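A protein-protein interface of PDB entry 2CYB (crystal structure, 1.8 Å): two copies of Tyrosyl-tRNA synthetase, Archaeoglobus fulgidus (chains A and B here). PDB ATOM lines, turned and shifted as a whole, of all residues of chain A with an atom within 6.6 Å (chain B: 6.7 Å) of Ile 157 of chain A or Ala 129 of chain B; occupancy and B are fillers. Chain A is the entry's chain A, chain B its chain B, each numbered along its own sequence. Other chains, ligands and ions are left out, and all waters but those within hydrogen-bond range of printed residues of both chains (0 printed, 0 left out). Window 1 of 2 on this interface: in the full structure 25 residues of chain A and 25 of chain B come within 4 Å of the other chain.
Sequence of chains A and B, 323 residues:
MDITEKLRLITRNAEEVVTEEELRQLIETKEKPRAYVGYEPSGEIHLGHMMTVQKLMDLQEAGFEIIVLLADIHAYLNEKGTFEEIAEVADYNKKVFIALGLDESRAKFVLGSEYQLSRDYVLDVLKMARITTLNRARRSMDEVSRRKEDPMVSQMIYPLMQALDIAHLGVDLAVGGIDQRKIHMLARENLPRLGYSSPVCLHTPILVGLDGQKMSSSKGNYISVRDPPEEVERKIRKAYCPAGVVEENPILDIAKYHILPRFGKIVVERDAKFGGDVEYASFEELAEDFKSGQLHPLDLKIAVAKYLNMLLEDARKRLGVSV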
ATOM      1  N   HIS A  74     -14.209  23.691 -12.465  1.00  0.00           N
ATOM      2  CA  HIS A  74     -13.401  24.897 -12.654  1.00  0.00           C
ATOM      3  C   HIS A  74     -12.160  24.595 -13.493  1.00  0.00           C
ATOM      4  O   HIS A  74     -11.794  25.371 -14.385  1.00  0.00           O
ATOM      5  CB  HIS A  74     -12.981  25.495 -11.309  1.00  0.00           C
ATOM      6  CG  HIS A  74     -14.053  26.310 -10.661  1.00  0.00           C
ATOM      7  ND1 HIS A  74     -15.088  25.746  -9.947  1.00  0.00           N
ATOM      8  CD2 HIS A  74     -14.279  27.646 -10.665  1.00  0.00           C
ATOM      9  CE1 HIS A  74     -15.905  26.701  -9.536  1.00  0.00           C
ATOM     10  NE2 HIS A  74     -15.438  27.862  -9.958  1.00  0.00           N
ATOM     11  N   LEU A  77     -13.210  24.396 -17.040  1.00  0.00           N
ATOM     12  CA  LEU A  77     -13.482  25.723 -17.587  1.00  0.00           C
ATOM     13  C   LEU A  77     -12.210  26.509 -17.853  1.00  0.00           C
ATOM     14  O   LEU A  77     -12.176  27.384 -18.725  1.00  0.00           O
ATOM     15  CB  LEU A  77     -14.327  26.527 -16.609  1.00  0.00           C
ATOM     16  CG  LEU A  77     -15.723  26.031 -16.262  1.00  0.00           C
ATOM     17  CD1 LEU A  77     -16.304  26.967 -15.200  1.00  0.00           C
ATOM     18  CD2 LEU A  77     -16.594  26.006 -17.521  1.00  0.00           C
ATOM     19  N   VAL A 125     -26.178  30.435 -10.672  1.00  0.00           N
ATOM     20  CA  VAL A 125     -25.161  30.878 -11.622  1.00  0.00           C
ATOM     21  C   VAL A 125     -25.799  31.855 -12.595  1.00  0.00           C
ATOM     22  O   VAL A 125     -25.232  32.911 -12.895  1.00  0.00           O
ATOM     23  CB  VAL A 125     -24.555  29.689 -12.420  1.00  0.00           C
ATOM     24  CG1 VAL A 125     -23.704  30.214 -13.578  1.00  0.00           C
ATOM     25  CG2 VAL A 125     -23.706  28.833 -11.504  1.00  0.00           C
ATOM     26  N   ALA A 137     -16.337  40.579 -14.114  1.00  0.00           N
ATOM     27  CA  ALA A 137     -15.963  39.175 -14.179  1.00  0.00           C
ATOM     28  C   ALA A 137     -14.597  38.993 -14.831  1.00  0.00           C
ATOM     29  O   ALA A 137     -13.740  38.259 -14.328  1.00  0.00           O
ATOM     30  CB  ALA A 137     -17.014  38.400 -14.957  1.00  0.00           C
ATOM     31  N   MET A 141     -10.697  37.720 -13.113  1.00  0.00           N
ATOM     32  CA  MET A 141      -9.940  36.582 -13.620  1.00  0.00           C
ATOM     33  C   MET A 141      -8.557  36.904 -14.177  1.00  0.00           C
ATOM     34  O   MET A 141      -7.868  36.009 -14.658  1.00  0.00           O
ATOM     35  CB  MET A 141     -10.753  35.872 -14.703  1.00  0.00           C
ATOM     36  CG  MET A 141     -12.008  35.176 -14.183  1.00  0.00           C
ATOM     37  SD  MET A 141     -11.546  33.816 -13.140  1.00  0.00           S
ATOM     38  CE  MET A 141     -10.900  32.721 -14.334  1.00  0.00           C
ATOM     39  N   MET A 152     -11.917  32.442 -23.034  1.00  0.00           N
ATOM     40  CA  MET A 152     -13.087  31.694 -23.488  1.00  0.00           C
ATOM     41  C   MET A 152     -14.250  32.125 -22.597  1.00  0.00           C
ATOM     42  O   MET A 152     -14.029  32.648 -21.498  1.00  0.00           O
ATOM     43  CB  MET A 152     -12.853  30.186 -23.316  1.00  0.00           C
ATOM     44  CG  MET A 152     -11.539  29.688 -23.885  1.00  0.00           C
ATOM     45  SD  MET A 152     -11.391  30.164 -25.623  1.00  0.00           S
ATOM     46  CE  MET A 152     -12.568  29.227 -26.307  1.00  0.00           C
ATOM     47  N   VAL A 153     -15.487  31.924 -23.051  1.00  0.00           N
ATOM     48  CA  VAL A 153     -16.623  32.295 -22.216  1.00  0.00           C
ATOM     49  C   VAL A 153     -16.563  31.506 -20.905  1.00  0.00           C
ATOM     50  O   VAL A 153     -16.977  32.000 -19.848  1.00  0.00           O
ATOM     51  CB  VAL A 153     -17.989  32.023 -22.919  1.00  0.00           C
ATOM     52  CG1 VAL A 153     -19.150  32.382 -21.969  1.00  0.00           C
ATOM     53  CG2 VAL A 153     -18.092  32.846 -24.209  1.00  0.00           C
ATOM     54  N   SER A 154     -16.031  30.289 -20.966  1.00  0.00           N
ATOM     55  CA  SER A 154     -15.947  29.460 -19.768  1.00  0.00           C
ATOM     56  C   SER A 154     -15.169  30.154 -18.650  1.00  0.00           C
ATOM     57  O   SER A 154     -15.453  29.952 -17.483  1.00  0.00           O
ATOM     58  CB  SER A 154     -15.296  28.111 -20.087  1.00  0.00           C
ATOM     59  OG  SER A 154     -13.979  28.283 -20.595  1.00  0.00           O
ATOM     60  N   GLN A 155     -14.204  30.994 -19.003  1.00  0.00           N
ATOM     61  CA  GLN A 155     -13.417  31.661 -17.978  1.00  0.00           C
ATOM     62  C   GLN A 155     -14.154  32.851 -17.359  1.00  0.00           C
ATOM     63  O   GLN A 155     -13.754  33.366 -16.315  1.00  0.00           O
ATOM     64  CB  GLN A 155     -12.043  32.032 -18.567  1.00  0.00           C
ATOM     65  CG  GLN A 155     -11.202  30.768 -18.826  1.00  0.00           C
ATOM     66  CD  GLN A 155     -10.175  30.904 -19.944  1.00  0.00           C
ATOM     67  OE1 GLN A 155     -10.411  31.570 -20.949  1.00  0.00           O
ATOM     68  NE2 GLN A 155      -9.036  30.239 -19.780  1.00  0.00           N
ATOM     69  N   MET A 156     -15.264  33.252 -17.972  1.00  0.00           N
ATOM     70  CA  MET A 156     -16.061  34.358 -17.445  1.00  0.00           C
ATOM     71  C   MET A 156     -17.156  33.818 -16.524  1.00  0.00           C
ATOM     72  O   MET A 156     -17.711  34.551 -15.706  1.00  0.00           O
ATOM     73  CB  MET A 156     -16.678  35.167 -18.590  1.00  0.00           C
ATOM     74  CG  MET A 156     -15.649  35.734 -19.560  1.00  0.00           C
ATOM     75  SD  MET A 156     -14.525  36.934 -18.775  1.00  0.00           S
ATOM     76  CE  MET A 156     -13.081  35.891 -18.429  1.00  0.00           C
ATOM     77  N   ILE A 157     -17.474  32.533 -16.674  1.00  0.00           N
ATOM     78  CA  ILE A 157     -18.473  31.875 -15.831  1.00  0.00           C
ATOM     79  C   ILE A 157     -17.772  31.438 -14.534  1.00  0.00           C
ATOM     80  O   ILE A 157     -18.354  31.478 -13.452  1.00  0.00           O
ATOM     81  CB  ILE A 157     -19.039  30.613 -16.524  1.00  0.00           C
ATOM     82  CG1 ILE A 157     -19.847  31.014 -17.759  1.00  0.00           C
ATOM     83  CG2 ILE A 157     -19.898  29.813 -15.548  1.00  0.00           C
ATOM     84  CD1 ILE A 157     -20.223  29.830 -18.635  1.00  0.00           C
ATOM     85  N   TYR A 158     -16.513  31.027 -14.681  1.00  0.00           N
ATOM     86  CA  TYR A 158     -15.637  30.561 -13.596  1.00  0.00           C
ATOM     87  C   TYR A 158     -15.715  31.356 -12.269  1.00  0.00           C
ATOM     88  O   TYR A 158     -15.960  30.773 -11.210  1.00  0.00           O
ATOM     89  CB  TYR A 158     -14.195  30.529 -14.148  1.00  0.00           C
ATOM     90  CG  TYR A 158     -13.101  29.999 -13.249  1.00  0.00           C
ATOM     91  CD1 TYR A 158     -12.351  28.871 -13.617  1.00  0.00           C
ATOM     92  CD2 TYR A 158     -12.754  30.665 -12.076  1.00  0.00           C
ATOM     93  CE1 TYR A 158     -11.278  28.434 -12.835  1.00  0.00           C
ATOM     94  CE2 TYR A 158     -11.693  30.239 -11.293  1.00  0.00           C
ATOM     95  CZ  TYR A 158     -10.962  29.129 -11.670  1.00  0.00           C
ATOM     96  OH  TYR A 158      -9.934  28.708 -10.862  1.00  0.00           O
ATOM     97  N   PRO A 159     -15.528  32.692 -12.304  1.00  0.00           N
ATOM     98  CA  PRO A 159     -15.594  33.459 -11.050  1.00  0.00           C
ATOM     99  C   PRO A 159     -16.950  33.427 -10.362  1.00  0.00           C
ATOM    100  O   PRO A 159     -17.028  33.407  -9.139  1.00  0.00           O
ATOM    101  CB  PRO A 159     -15.196  34.875 -11.480  1.00  0.00           C
ATOM    102  CG  PRO A 159     -15.711  34.940 -12.901  1.00  0.00           C
ATOM    103  CD  PRO A 159     -15.306  33.586 -13.455  1.00  0.00           C
ATOM    104  N   LEU A 160     -18.015  33.422 -11.148  1.00  0.00           N
ATOM    105  CA  LEU A 160     -19.355  33.374 -10.585  1.00  0.00           C
ATOM    106  C   LEU A 160     -19.542  32.078  -9.798  1.00  0.00           C
ATOM    107  O   LEU A 160     -20.105  32.075  -8.701  1.00  0.00           O
ATOM    108  CB  LEU A 160     -20.399  33.450 -11.698  1.00  0.00           C
ATOM    109  CG  LEU A 160     -20.212  34.568 -12.726  1.00  0.00           C
ATOM    110  CD1 LEU A 160     -21.383  34.539 -13.702  1.00  0.00           C
ATOM    111  CD2 LEU A 160     -20.123  35.919 -12.027  1.00  0.00           C
ATOM    112  N   MET A 161     -19.061  30.980 -10.367  1.00  0.00           N
ATOM    113  CA  MET A 161     -19.182  29.683  -9.732  1.00  0.00           C
ATOM    114  C   MET A 161     -18.333  29.592  -8.482  1.00  0.00           C
ATOM    115  O   MET A 161     -18.734  28.957  -7.518  1.00  0.00           O
ATOM    116  CB  MET A 161     -18.806  28.575 -10.714  1.00  0.00           C
ATOM    117  CG  MET A 161     -19.893  28.302 -11.744  1.00  0.00           C
ATOM    118  SD  MET A 161     -19.416  26.977 -12.862  1.00  0.00           S
ATOM    119  CE  MET A 161     -19.123  25.613 -11.711  1.00  0.00           C
ATOM    120  N   GLN A 162     -17.157  30.210  -8.499  1.00  0.00           N
ATOM    121  CA  GLN A 162     -16.302  30.190  -7.320  1.00  0.00           C
ATOM    122  C   GLN A 162     -17.013  30.906  -6.177  1.00  0.00           C
ATOM    123  O   GLN A 162     -17.034  30.419  -5.047  1.00  0.00           O
ATOM    124  CB  GLN A 162     -14.964  30.878  -7.596  1.00  0.00           C
ATOM    125  CG  GLN A 162     -14.027  30.841  -6.401  1.00  0.00           C
ATOM    126  CD  GLN A 162     -12.601  31.181  -6.779  1.00  0.00           C
ATOM    127  OE1 GLN A 162     -12.176  30.941  -7.910  1.00  0.00           O
ATOM    128  NE2 GLN A 162     -11.846  31.718  -5.826  1.00  0.00           N
ATOM    129  N   ASP B 124     -23.561  20.681 -21.418  1.00  0.00           N
ATOM    130  CA  ASP B 124     -23.262  21.113 -22.780  1.00  0.00           C
ATOM    131  C   ASP B 124     -22.964  22.611 -22.801  1.00  0.00           C
ATOM    132  O   ASP B 124     -22.137  23.060 -23.586  1.00  0.00           O
ATOM    133  CB  ASP B 124     -24.422  20.805 -23.740  1.00  0.00           C
ATOM    134  CG  ASP B 124     -24.352  19.400 -24.303  1.00  0.00           C
ATOM    135  OD1 ASP B 124     -25.321  18.972 -24.963  1.00  0.00           O
ATOM    136  OD2 ASP B 124     -23.318  18.725 -24.092  1.00  0.00           O
ATOM    137  N   VAL B 125     -23.639  23.374 -21.946  1.00  0.00           N
ATOM    138  CA  VAL B 125     -23.378  24.814 -21.897  1.00  0.00           C
ATOM    139  C   VAL B 125     -21.913  25.038 -21.481  1.00  0.00           C
ATOM    140  O   VAL B 125     -21.219  25.895 -22.047  1.00  0.00           O
ATOM    141  CB  VAL B 125     -24.333  25.532 -20.905  1.00  0.00           C
ATOM    142  CG1 VAL B 125     -23.883  26.968 -20.693  1.00  0.00           C
ATOM    143  CG2 VAL B 125     -25.767  25.523 -21.448  1.00  0.00           C
ATOM    144  N   LEU B 126     -21.441  24.264 -20.503  1.00  0.00           N
ATOM    145  CA  LEU B 126     -20.059  24.382 -20.034  1.00  0.00           C
ATOM    146  C   LEU B 126     -19.082  23.970 -21.137  1.00  0.00           C
ATOM    147  O   LEU B 126     -18.024  24.577 -21.311  1.00  0.00           O
ATOM    148  CB  LEU B 126     -19.832  23.521 -18.774  1.00  0.00           C
ATOM    149  CG  LEU B 126     -20.639  23.923 -17.527  1.00  0.00           C
ATOM    150  CD1 LEU B 126     -20.150  23.111 -16.349  1.00  0.00           C
ATOM    151  CD2 LEU B 126     -20.490  25.421 -17.241  1.00  0.00           C
ATOM    152  N   LYS B 127     -19.438  22.935 -21.888  1.00  0.00           N
ATOM    153  CA  LYS B 127     -18.591  22.484 -22.983  1.00  0.00           C
ATOM    154  C   LYS B 127     -18.560  23.543 -24.089  1.00  0.00           C
ATOM    155  O   LYS B 127     -17.505  23.823 -24.667  1.00  0.00           O
ATOM    156  CB  LYS B 127     -19.109  21.165 -23.552  1.00  0.00           C
ATOM    157  CG  LYS B 127     -18.981  19.974 -22.605  1.00  0.00           C
ATOM    158  CD  LYS B 127     -19.588  18.719 -23.241  1.00  0.00           C
ATOM    159  CE  LYS B 127     -19.112  17.461 -22.536  1.00  0.00           C
ATOM    160  NZ  LYS B 127     -19.319  17.542 -21.071  1.00  0.00           N
ATOM    161  N   MET B 128     -19.717  24.132 -24.380  1.00  0.00           N
ATOM    162  CA  MET B 128     -19.800  25.158 -25.415  1.00  0.00           C
ATOM    163  C   MET B 128     -19.010  26.390 -24.972  1.00  0.00           C
ATOM    164  O   MET B 128     -18.331  27.035 -25.782  1.00  0.00           O
ATOM    165  CB  MET B 128     -21.270  25.527 -25.661  1.00  0.00           C
ATOM    166  CG  MET B 128     -21.508  26.470 -26.819  1.00  0.00           C
ATOM    167  SD  MET B 128     -21.021  25.742 -28.403  1.00  0.00           S
ATOM    168  CE  MET B 128     -22.318  24.602 -28.675  1.00  0.00           C
ATOM    169  N   ALA B 129     -19.089  26.715 -23.681  1.00  0.00           N
ATOM    170  CA  ALA B 129     -18.373  27.882 -23.151  1.00  0.00           C
ATOM    171  C   ALA B 129     -16.869  27.682 -23.256  1.00  0.00           C
ATOM    172  O   ALA B 129     -16.112  28.627 -23.488  1.00  0.00           O
ATOM    173  CB  ALA B 129     -18.762  28.130 -21.695  1.00  0.00           C
ATOM    174  N   ARG B 130     -16.452  26.433 -23.100  1.00  0.00           N
ATOM    175  CA  ARG B 130     -15.041  26.061 -23.159  1.00  0.00           C
ATOM    176  C   ARG B 130     -14.413  26.220 -24.542  1.00  0.00           C
ATOM    177  O   ARG B 130     -13.211  26.480 -24.655  1.00  0.00           O
ATOM    178  CB  ARG B 130     -14.882  24.604 -22.699  1.00  0.00           C
ATOM    179  CG  ARG B 130     -13.522  23.983 -22.989  1.00  0.00           C
ATOM    180  CD  ARG B 130     -12.436  24.576 -22.131  1.00  0.00           C
ATOM    181  NE  ARG B 130     -11.135  23.957 -22.394  1.00  0.00           N
ATOM    182  CZ  ARG B 130     -10.417  24.147 -23.498  1.00  0.00           C
ATOM    183  NH1 ARG B 130     -10.863  24.941 -24.465  1.00  0.00           N
ATOM    184  NH2 ARG B 130      -9.239  23.547 -23.630  1.00  0.00           N
ATOM    185  N   ILE B 131     -15.211  26.050 -25.592  1.00  0.00           N
ATOM    186  CA  ILE B 131     -14.680  26.169 -26.945  1.00  0.00           C
ATOM    187  C   ILE B 131     -15.119  27.428 -27.685  1.00  0.00           C
ATOM    188  O   ILE B 131     -14.818  27.593 -28.866  1.00  0.00           O
ATOM    189  CB  ILE B 131     -15.064  24.949 -27.812  1.00  0.00           C
ATOM    190  CG1 ILE B 131     -16.579  24.887 -27.996  1.00  0.00           C
ATOM    191  CG2 ILE B 131     -14.544  23.672 -27.163  1.00  0.00           C
ATOM    192  CD1 ILE B 131     -17.005  23.869 -29.060  1.00  0.00           C
ATOM    193  N   THR B 132     -15.834  28.314 -27.004  1.00  0.00           N
ATOM    194  CA  THR B 132     -16.281  29.549 -27.646  1.00  0.00           C
ATOM    195  C   THR B 132     -15.562  30.748 -27.032  1.00  0.00           C
ATOM    196  O   THR B 132     -15.618  30.958 -25.819  1.00  0.00           O
ATOM    197  CB  THR B 132     -17.798  29.748 -27.484  1.00  0.00           C
ATOM    198  OG1 THR B 132     -18.498  28.608 -28.005  1.00  0.00           O
ATOM    199  CG2 THR B 132     -18.241  30.992 -28.234  1.00  0.00           C
ATOM    200  N   THR B 133     -14.888  31.545 -27.857  1.00  0.00           N
ATOM    201  CA  THR B 133     -14.175  32.699 -27.315  1.00  0.00           C
ATOM    202  C   THR B 133     -15.141  33.784 -26.855  1.00  0.00           C
ATOM    203  O   THR B 133     -16.226  33.952 -27.410  1.00  0.00           O
ATOM    204  CB  THR B 133     -13.184  33.327 -28.348  1.00  0.00           C
ATOM    205  OG1 THR B 133     -13.913  33.888 -29.444  1.00  0.00           O
ATOM    206  CG2 THR B 133     -12.215  32.263 -28.873  1.00  0.00           C
ATOM    207  N   LEU B 134     -14.754  34.517 -25.819  1.00  0.00           N
ATOM    208  CA  LEU B 134     -15.612  35.586 -25.344  1.00  0.00           C
ATOM    209  C   LEU B 134     -15.837  36.552 -26.494  1.00  0.00           C
ATOM    210  O   LEU B 134     -16.932  37.074 -26.677  1.00  0.00           O
ATOM    211  CB  LEU B 134     -14.961  36.324 -24.178  1.00  0.00           C
ATOM    212  CG  LEU B 134     -15.647  37.624 -23.743  1.00  0.00           C
ATOM    213  CD1 LEU B 134     -17.070  37.313 -23.219  1.00  0.00           C
ATOM    214  CD2 LEU B 134     -14.815  38.307 -22.661  1.00  0.00           C
ATOM    215  N   VAL B 153     -22.588  39.189 -17.749  1.00  0.00           N
ATOM    216  CA  VAL B 153     -22.055  37.877 -18.104  1.00  0.00           C
ATOM    217  C   VAL B 153     -23.205  37.050 -18.682  1.00  0.00           C
ATOM    218  O   VAL B 153     -22.997  36.220 -19.576  1.00  0.00           O
ATOM    219  CB  VAL B 153     -21.461  37.145 -16.872  1.00  0.00           C
ATOM    220  CG1 VAL B 153     -21.008  35.733 -17.258  1.00  0.00           C
ATOM    221  CG2 VAL B 153     -20.260  37.942 -16.318  1.00  0.00           C
ATOM    222  N   ILE B 157     -23.546  34.221 -22.048  1.00  0.00           N
ATOM    223  CA  ILE B 157     -23.989  32.830 -21.915  1.00  0.00           C
ATOM    224  C   ILE B 157     -25.122  32.588 -22.912  1.00  0.00           C
ATOM    225  O   ILE B 157     -25.251  31.508 -23.495  1.00  0.00           O
ATOM    226  CB  ILE B 157     -24.532  32.529 -20.487  1.00  0.00           C
ATOM    227  CG1 ILE B 157     -23.380  32.503 -19.480  1.00  0.00           C
ATOM    228  CG2 ILE B 157     -25.260  31.176 -20.479  1.00  0.00           C
ATOM    229  CD1 ILE B 157     -23.842  32.357 -18.035  1.00  0.00           C
ATOM    230  N   LEU B 160     -24.603  30.842 -26.383  1.00  0.00           N
ATOM    231  CA  LEU B 160     -24.215  29.435 -26.234  1.00  0.00           C
ATOM    232  C   LEU B 160     -25.483  28.594 -26.060  1.00  0.00           C
ATOM    233  O   LEU B 160     -25.623  27.520 -26.664  1.00  0.00           O
ATOM    234  CB  LEU B 160     -23.319  29.245 -25.005  1.00  0.00           C
ATOM    235  CG  LEU B 160     -21.801  29.435 -25.115  1.00  0.00           C
ATOM    236  CD1 LEU B 160     -21.442  30.519 -26.098  1.00  0.00           C
ATOM    237  CD2 LEU B 160     -21.243  29.724 -23.728  1.00  0.00           C
ATOM    238  N   LEU B 164     -27.235  25.659 -28.391  1.00  0.00           N
ATOM    239  CA  LEU B 164     -27.563  24.337 -27.820  1.00  0.00           C
ATOM    240  C   LEU B 164     -29.042  23.981 -27.903  1.00  0.00           C
ATOM    241  O   LEU B 164     -29.381  22.797 -27.954  1.00  0.00           O
ATOM    242  CB  LEU B 164     -27.085  24.242 -26.370  1.00  0.00           C
ATOM    243  CG  LEU B 164     -25.568  24.093 -26.254  1.00  0.00           C
ATOM    244  CD1 LEU B 164     -25.117  24.389 -24.840  1.00  0.00           C
ATOM    245  CD2 LEU B 164     -25.173  22.691 -26.688  1.00  0.00           C
ATOM    246  N   LEU B 194     -19.215  19.366 -30.532  1.00  0.00           N
ATOM    247  CA  LEU B 194     -19.783  18.726 -29.359  1.00  0.00           C
ATOM    248  C   LEU B 194     -20.452  17.418 -29.767  1.00  0.00           C
ATOM    249  O   LEU B 194     -21.105  16.765 -28.952  1.00  0.00           O
ATOM    250  CB  LEU B 194     -20.809  19.633 -28.669  1.00  0.00           C
ATOM    251  CG  LEU B 194     -20.234  20.674 -27.704  1.00  0.00           C
ATOM    252  CD1 LEU B 194     -19.417  21.691 -28.461  1.00  0.00           C
ATOM    253  CD2 LEU B 194     -21.377  21.364 -26.958  1.00  0.00           C
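Val 153 of chain A touches Leu 160 of chain B, and with the chains exchanged Leu 160 of chain A touches Val 153 of chain B.
Of chain B, only Ala 129 comes within 4 Å of Ile 157 of chain A.
Ala 129 of chain B touches four residues of chain A.
Printed residues of chain A within 4 Å of Leu 134 of chain B: Val 153 (3.9 Å).
Of the printed residues of chain A, Leu 160 of chain B touches Val 153.
Val 125 of chain B touches none of the printed residues of chain A.
Gln 155 of chain A touches none of the printed residues of chain B.
The nearest residue of chain B that does not touch Ile 157 of chain A is Ile 157 of chain B (4.2 Å).
The nearest printed residue of chain A that does not touch Leu 134 of chain B is Met 152 of chain A (4.02 Å).
The backbone carbonyl oxygen (O) of Leu 77 of chain A sits at hydrogen-bond distance from the side-chain hydroxyl (OG) of Ser 154 of chain A (2.7 Å).
The side-chain hydroxyl (OG1) of Thr 132 of chain B sits at hydrogen-bond distance from the backbone carbonyl oxygen (O) of Met 128 of chain B, 2.7 Å away.
The side-chain amide oxygen (OE1) of Gln 155 of chain A is in hydrogen-bond range of the backbone NH (N) of Met 152 of chain A.
Hydrophobic or aromatic side chains of chain A that line the printed part of chain B: Leu 77, Ala 137, Met 152, Val 153, Ile 157 and Leu 160.
Hydrophobic or aromatic side chains of chain B that line the printed part of chain A: Leu 126, Ala 129, Val 153 and Leu 160.
Among the printed residues, 17 pairs touch across the chains.
Among the printed residues, no Asp or Glu carboxylate lies within 4 Å of a Lys or Arg side-chain nitrogen of the other chain.
The backbone carbonyl oxygen (O) of Ala 129 of chain B is in hydrogen-bond range of the backbone NH (N) of Ser 154 of chain A.
The backbone NH of Val 153 of chain A lies within hydrogen-bond range of the backbone carbonyl oxygen of Thr 132 of chain B, 2.9 Å away.
The backbone NH (N) of Val 153 of chain A lies within hydrogen-bond range of the backbone carbonyl oxygen (O) of Ala 129 of chain B, 3.4 Å away.
Among the printed residues, merely in contact across the chains: Met 152 of chain A with Arg 130 of chain B, Met 152 of chain A with Ile 131 of chain B, Met 152 of chain A with Thr 132 of chain B, Ala 137 of chain A with Val 153 of chain B, Ser 154 of chain A with Arg 130 of chain B, Met 152 of chain A with Ala 129 of chain B, Met 152 of chain A with Thr 133 of chain B, Leu 160 of chain A with Val 153 of chain B, Ile 157 of chain A with Ala 129 of chain B, Val 153 of chain A with Leu 160 of chain B, Met 156 of chain A with Val 153 of chain B, Val 153 of chain A with Leu 134 of chain B, Val 153 of chain A with Thr 133 of chain B and Leu 77 of chain A with Leu 126 of chain B.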
